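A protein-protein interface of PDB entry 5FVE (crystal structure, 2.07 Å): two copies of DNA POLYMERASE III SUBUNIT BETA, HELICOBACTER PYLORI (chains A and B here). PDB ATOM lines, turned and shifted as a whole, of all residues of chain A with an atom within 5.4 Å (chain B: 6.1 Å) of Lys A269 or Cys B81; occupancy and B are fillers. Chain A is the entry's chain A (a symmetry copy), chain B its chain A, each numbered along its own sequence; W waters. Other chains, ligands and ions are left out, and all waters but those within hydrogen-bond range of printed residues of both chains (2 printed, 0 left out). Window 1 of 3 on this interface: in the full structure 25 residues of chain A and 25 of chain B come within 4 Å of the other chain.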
ATOM      1  N   PHE A 264      -1.066  35.488   9.254  1.00  0.00           N
ATOM      2  CA  PHE A 264      -0.805  34.155   9.793  1.00  0.00           C
ATOM      3  C   PHE A 264      -1.652  33.074   9.094  1.00  0.00           C
ATOM      4  O   PHE A 264      -1.147  31.996   8.842  1.00  0.00           O
ATOM      5  CB  PHE A 264      -0.986  34.100  11.325  1.00  0.00           C
ATOM      6  CG  PHE A 264       0.277  34.428  12.090  1.00  0.00           C
ATOM      7  CD1 PHE A 264       0.846  35.683  11.989  1.00  0.00           C
ATOM      8  CD2 PHE A 264       0.921  33.463  12.860  1.00  0.00           C
ATOM      9  CE1 PHE A 264       2.037  35.994  12.663  1.00  0.00           C
ATOM     10  CE2 PHE A 264       2.094  33.766  13.541  1.00  0.00           C
ATOM     11  CZ  PHE A 264       2.661  35.034  13.433  1.00  0.00           C
ATOM     12  N   LYS A 265      -2.922  33.360   8.801  1.00  0.00           N
ATOM     13  CA  LYS A 265      -3.759  32.419   8.030  1.00  0.00           C
ATOM     14  C   LYS A 265      -3.117  32.056   6.705  1.00  0.00           C
ATOM     15  O   LYS A 265      -2.981  30.877   6.383  1.00  0.00           O
ATOM     16  CB  LYS A 265      -5.135  32.991   7.721  1.00  0.00           C
ATOM     17  CG  LYS A 265      -6.130  32.884   8.848  1.00  0.00           C
ATOM     18  CD  LYS A 265      -7.519  33.233   8.335  1.00  0.00           C
ATOM     19  CE  LYS A 265      -8.443  33.544   9.497  1.00  0.00           C
ATOM     20  NZ  LYS A 265      -9.843  33.755   9.031  1.00  0.00           N
ATOM     21  N   GLU A 266      -2.734  33.083   5.947  1.00  0.00           N
ATOM     22  CA  GLU A 266      -2.154  32.885   4.613  1.00  0.00           C
ATOM     23  C   GLU A 266      -0.851  32.125   4.704  1.00  0.00           C
ATOM     24  O   GLU A 266      -0.595  31.232   3.906  1.00  0.00           O
ATOM     25  CB  GLU A 266      -1.910  34.220   3.902  1.00  0.00           C
ATOM     26  CG  GLU A 266      -3.200  34.958   3.595  1.00  0.00           C
ATOM     27  CD  GLU A 266      -2.987  36.348   3.018  1.00  0.00           C
ATOM     28  OE1 GLU A 266      -1.831  36.714   2.674  1.00  0.00           O
ATOM     29  OE2 GLU A 266      -4.011  37.070   2.902  1.00  0.00           O
ATOM     30  N   SER A 267      -0.026  32.472   5.688  1.00  0.00           N
ATOM     31  CA  SER A 267       1.277  31.848   5.823  1.00  0.00           C
ATOM     32  C   SER A 267       1.139  30.379   6.202  1.00  0.00           C
ATOM     33  O   SER A 267       1.900  29.528   5.734  1.00  0.00           O
ATOM     34  CB  SER A 267       2.127  32.598   6.851  1.00  0.00           C
ATOM     35  OG  SER A 267       2.264  33.955   6.458  1.00  0.00           O
ATOM     36  N   ILE A 268       0.151  30.079   7.031  1.00  0.00           N
ATOM     37  CA  ILE A 268      -0.054  28.711   7.492  1.00  0.00           C
ATOM     38  C   ILE A 268      -0.665  27.860   6.385  1.00  0.00           C
ATOM     39  O   ILE A 268      -0.212  26.745   6.169  1.00  0.00           O
ATOM     40  CB  ILE A 268      -0.870  28.677   8.795  1.00  0.00           C
ATOM     41  CG1 ILE A 268       0.018  29.186   9.949  1.00  0.00           C
ATOM     42  CG2 ILE A 268      -1.358  27.263   9.109  1.00  0.00           C
ATOM     43  CD1 ILE A 268      -0.742  29.691  11.139  1.00  0.00           C
ATOM     44  N   LYS A 269      -1.692  28.379   5.714  1.00  0.00           N
ATOM     45  CA  LYS A 269      -2.276  27.698   4.549  1.00  0.00           C
ATOM     46  C   LYS A 269      -1.175  27.366   3.562  1.00  0.00           C
ATOM     47  O   LYS A 269      -1.055  26.234   3.126  1.00  0.00           O
ATOM     48  CB  LYS A 269      -3.338  28.560   3.871  1.00  0.00           C
ATOM     49  CG  LYS A 269      -4.649  28.558   4.618  1.00  0.00           C
ATOM     50  CD  LYS A 269      -5.654  29.528   4.010  1.00  0.00           C
ATOM     51  CE  LYS A 269      -6.770  29.812   4.999  1.00  0.00           C
ATOM     52  NZ  LYS A 269      -7.789  30.775   4.477  1.00  0.00           N
ATOM     53  N   LEU A 270      -0.339  28.357   3.278  1.00  0.00           N
ATOM     54  CA  LEU A 270       0.749  28.207   2.340  1.00  0.00           C
ATOM     55  C   LEU A 270       1.657  27.044   2.724  1.00  0.00           C
ATOM     56  O   LEU A 270       1.885  26.164   1.890  1.00  0.00           O
ATOM     57  CB  LEU A 270       1.514  29.526   2.203  1.00  0.00           C
ATOM     58  CG  LEU A 270       2.666  29.585   1.213  1.00  0.00           C
ATOM     59  CD1 LEU A 270       2.749  30.940   0.529  1.00  0.00           C
ATOM     60  CD2 LEU A 270       3.984  29.263   1.891  1.00  0.00           C
ATOM     61  N   CYS A 271       2.140  27.005   3.974  1.00  0.00           N
ATOM     62  CA  CYS A 271       3.058  25.930   4.390  1.00  0.00           C
ATOM     63  C   CYS A 271       2.349  24.588   4.497  1.00  0.00           C
ATOM     64  O   CYS A 271       2.964  23.550   4.287  1.00  0.00           O
ATOM     65  CB  CYS A 271       3.789  26.271   5.689  1.00  0.00           C
ATOM     66  SG  CYS A 271       4.900  27.671   5.478  1.00  0.00           S
ATOM     67  N   SER A 272       1.049  24.617   4.764  1.00  0.00           N
ATOM     68  CA  SER A 272       0.268  23.399   4.861  1.00  0.00           C
ATOM     69  C   SER A 272      -0.045  22.747   3.499  1.00  0.00           C
ATOM     70  O   SER A 272      -0.597  21.659   3.464  1.00  0.00           O
ATOM     71  CB  SER A 272      -1.021  23.643   5.648  1.00  0.00           C
ATOM     72  OG  SER A 272      -1.897  24.470   4.922  1.00  0.00           O
ATOM     73  N   SER A 273       0.298  23.397   2.388  1.00  0.00           N
ATOM     74  CA  SER A 273       0.283  22.726   1.087  1.00  0.00           C
ATOM     75  C   SER A 273       1.170  21.461   1.074  1.00  0.00           C
ATOM     76  O   SER A 273       0.844  20.502   0.385  1.00  0.00           O
ATOM     77  CB  SER A 273       0.683  23.688  -0.036  1.00  0.00           C
ATOM     78  OG  SER A 273       2.021  24.126   0.103  1.00  0.00           O
ATOM     79  N   LEU A 326      -5.216  27.327  12.342  1.00  0.00           N
ATOM     80  CA  LEU A 326      -6.140  28.005  11.428  1.00  0.00           C
ATOM     81  C   LEU A 326      -7.539  28.094  11.975  1.00  0.00           C
ATOM     82  O   LEU A 326      -8.147  29.171  11.951  1.00  0.00           O
ATOM     83  CB  LEU A 326      -6.205  27.293  10.074  1.00  0.00           C
ATOM     84  CG  LEU A 326      -4.989  27.442   9.187  1.00  0.00           C
ATOM     85  CD1 LEU A 326      -5.232  26.641   7.911  1.00  0.00           C
ATOM     86  CD2 LEU A 326      -4.730  28.911   8.874  1.00  0.00           C
ATOM     87  N   LYS B   7       1.838  33.770 -12.456  1.00  0.00           N
ATOM     88  CA  LYS B   7       1.155  32.856 -11.534  1.00  0.00           C
ATOM     89  C   LYS B   7      -0.131  32.283 -12.123  1.00  0.00           C
ATOM     90  O   LYS B   7      -0.335  31.075 -12.075  1.00  0.00           O
ATOM     91  CB  LYS B   7       0.885  33.560 -10.205  1.00  0.00           C
ATOM     92  CG  LYS B   7       0.229  32.699  -9.123  1.00  0.00           C
ATOM     93  CD  LYS B   7      -1.289  32.772  -9.125  1.00  0.00           C
ATOM     94  CE  LYS B   7      -1.857  32.607  -7.728  1.00  0.00           C
ATOM     95  NZ  LYS B   7      -3.296  32.223  -7.772  1.00  0.00           N
ATOM     96  N   LEU B  76       0.577  22.266  -8.124  1.00  0.00           N
ATOM     97  CA  LEU B  76      -0.676  23.028  -8.150  1.00  0.00           C
ATOM     98  C   LEU B  76      -1.092  23.516  -6.762  1.00  0.00           C
ATOM     99  O   LEU B  76      -1.532  24.652  -6.630  1.00  0.00           O
ATOM    100  CB  LEU B  76      -1.815  22.220  -8.779  1.00  0.00           C
ATOM    101  CG  LEU B  76      -3.203  22.881  -8.825  1.00  0.00           C
ATOM    102  CD1 LEU B  76      -3.200  24.273  -9.455  1.00  0.00           C
ATOM    103  CD2 LEU B  76      -4.166  21.980  -9.574  1.00  0.00           C
ATOM    104  N   ASP B  77      -0.940  22.679  -5.735  1.00  0.00           N
ATOM    105  CA  ASP B  77      -1.309  23.085  -4.368  1.00  0.00           C
ATOM    106  C   ASP B  77      -0.464  24.269  -3.907  1.00  0.00           C
ATOM    107  O   ASP B  77      -0.997  25.204  -3.328  1.00  0.00           O
ATOM    108  CB  ASP B  77      -1.182  21.931  -3.378  1.00  0.00           C
ATOM    109  CG  ASP B  77      -2.255  20.849  -3.563  1.00  0.00           C
ATOM    110  OD1 ASP B  77      -3.259  21.070  -4.257  1.00  0.00           O
ATOM    111  OD2 ASP B  77      -2.080  19.751  -3.013  1.00  0.00           O
ATOM    112  N   ILE B  78       0.841  24.245  -4.189  1.00  0.00           N
ATOM    113  CA  ILE B  78       1.721  25.382  -3.850  1.00  0.00           C
ATOM    114  C   ILE B  78       1.363  26.679  -4.583  1.00  0.00           C
ATOM    115  O   ILE B  78       1.253  27.723  -3.944  1.00  0.00           O
ATOM    116  CB  ILE B  78       3.210  25.057  -4.098  1.00  0.00           C
ATOM    117  CG1 ILE B  78       3.698  24.031  -3.072  1.00  0.00           C
ATOM    118  CG2 ILE B  78       4.082  26.313  -4.005  1.00  0.00           C
ATOM    119  CD1 ILE B  78       4.998  23.358  -3.458  1.00  0.00           C
ATOM    120  N   ILE B  79       1.195  26.614  -5.903  1.00  0.00           N
ATOM    121  CA  ILE B  79       0.950  27.811  -6.714  1.00  0.00           C
ATOM    122  C   ILE B  79      -0.388  28.473  -6.358  1.00  0.00           C
ATOM    123  O   ILE B  79      -0.472  29.708  -6.289  1.00  0.00           O
ATOM    124  CB  ILE B  79       0.992  27.519  -8.246  1.00  0.00           C
ATOM    125  CG1 ILE B  79       2.356  26.948  -8.693  1.00  0.00           C
ATOM    126  CG2 ILE B  79       0.653  28.773  -9.062  1.00  0.00           C
ATOM    127  CD1 ILE B  79       3.578  27.604  -8.094  1.00  0.00           C
ATOM    128  N   SER B  80      -1.411  27.648  -6.123  1.00  0.00           N
ATOM    129  CA  SER B  80      -2.715  28.109  -5.652  1.00  0.00           C
ATOM    130  C   SER B  80      -2.685  28.967  -4.388  1.00  0.00           C
ATOM    131  O   SER B  80      -3.548  29.821  -4.221  1.00  0.00           O
ATOM    132  CB  SER B  80      -3.633  26.913  -5.412  1.00  0.00           C
ATOM    133  OG  SER B  80      -3.918  26.290  -6.644  1.00  0.00           O
ATOM    134  N   CYS B  81      -1.723  28.720  -3.502  1.00  0.00           N
ATOM    135  CA  CYS B  81      -1.585  29.476  -2.251  1.00  0.00           C
ATOM    136  C   CYS B  81      -0.691  30.734  -2.377  1.00  0.00           C
ATOM    137  O   CYS B  81      -0.446  31.422  -1.384  1.00  0.00           O
ATOM    138  CB  CYS B  81      -1.085  28.544  -1.121  1.00  0.00           C
ATOM    139  SG  CYS B  81      -2.411  27.566  -0.359  1.00  0.00           S
ATOM    140  N   LEU B  82      -0.224  31.038  -3.586  1.00  0.00           N
ATOM    141  CA  LEU B  82       0.598  32.221  -3.833  1.00  0.00           C
ATOM    142  C   LEU B  82      -0.218  33.410  -4.337  1.00  0.00           C
ATOM    143  O   LEU B  82      -1.375  33.278  -4.746  1.00  0.00           O
ATOM    144  CB  LEU B  82       1.718  31.899  -4.832  1.00  0.00           C
ATOM    145  CG  LEU B  82       2.749  30.893  -4.310  1.00  0.00           C
ATOM    146  CD1 LEU B  82       3.800  30.581  -5.369  1.00  0.00           C
ATOM    147  CD2 LEU B  82       3.406  31.397  -3.039  1.00  0.00           C
ATOM    148  N   LYS B  83       0.424  34.573  -4.296  1.00  0.00           N
ATOM    149  CA  LYS B  83      -0.167  35.832  -4.760  1.00  0.00           C
ATOM    150  C   LYS B  83       0.063  35.978  -6.253  1.00  0.00           C
ATOM    151  O   LYS B  83       0.774  35.175  -6.848  1.00  0.00           O
ATOM    152  CB  LYS B  83       0.429  36.994  -3.970  1.00  0.00           C
ATOM    153  CG  LYS B  83       0.030  36.936  -2.501  1.00  0.00           C
ATOM    154  CD  LYS B  83       0.963  37.703  -1.589  1.00  0.00           C
ATOM    155  CE  LYS B  83       0.398  37.721  -0.178  1.00  0.00           C
ATOM    156  NZ  LYS B  83       1.288  38.434   0.775  1.00  0.00           N
HETATM  157  O   HOH W   1       0.371  19.195  -1.885  1.00  0.00           O
HETATM  158  O   HOH W   2      -2.111  31.291   1.512  1.00  0.00           O
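The backbone carbonyl oxygen (O) of Lys A269 is in hydrogen-bond range of the side-chain hydroxyl (OG) of Ser A272 (2.7 Å). O of Leu A270 sits at hydrogen-bond distance from OG of Ser A273 (2.7 Å).
Among the printed residues, pairs that only touch across the chains: Glu A266 with Lys B83 (3.8 Å), Lys A269 with Cys B81 (3.97 Å), Leu A270 with Cys B81 (3.8 Å), Leu A270 with Leu B82 (3.7 Å), Ser A273 with Asp B77 (3.99 Å) and Ser A273 with Ile B78 (3.6 Å).
Of the printed residues of chain B, Glu A266 touches Lys B83. Of the printed residues of chain B, Ser A273 touches Asp B77 (3.99 Å) and Ile B78 (3.6 Å). Of the printed residues of chain A, Asp B77 touches Ser A273. Ile B79 touches none of the printed residues of chain A. Of chain A, only Lys A269 and Leu A270 come within 4 Å of Cys B81. Of the printed residues of chain A, Leu B82 touches Leu A270 (3.7 Å). Of the printed residues of chain A, Lys B83 touches Glu A266 (3.8 Å). The nearest residue of chain A that does not touch Cys B81 is Ser A273 (5.0 Å). The nearest printed residue of chain A that does not touch Lys B83 is Leu A270 (6.5 Å).
Of the 11 printed residues of chain A, 4 touch a printed residue of chain B. Printed residues of chain B that touch a printed residue of chain A: Asp B77, Ile B78, Cys B81, Leu B82 and Lys B83. Hydrophobic or aromatic side chains of chain B that line the printed part of chain A: Ile B78 and Leu B82. Along chain B the printed residues that touch a printed residue of chain A span positions 77 to 83.
No position is printed for both chains. Of the 6 pairs that touch across the chains among the printed residues, none has its exchanged pair printed and touching as well.
Water W1 lies within hydrogen-bond range of O of Ser A273 (2.7 Å) and OD2 of Asp B77 (2.8 Å). Water W2 bridges the backbone carbonyl oxygen of Glu A266 (2.8 Å) and the backbone carbonyl oxygen of Cys B81 (3.3 Å).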
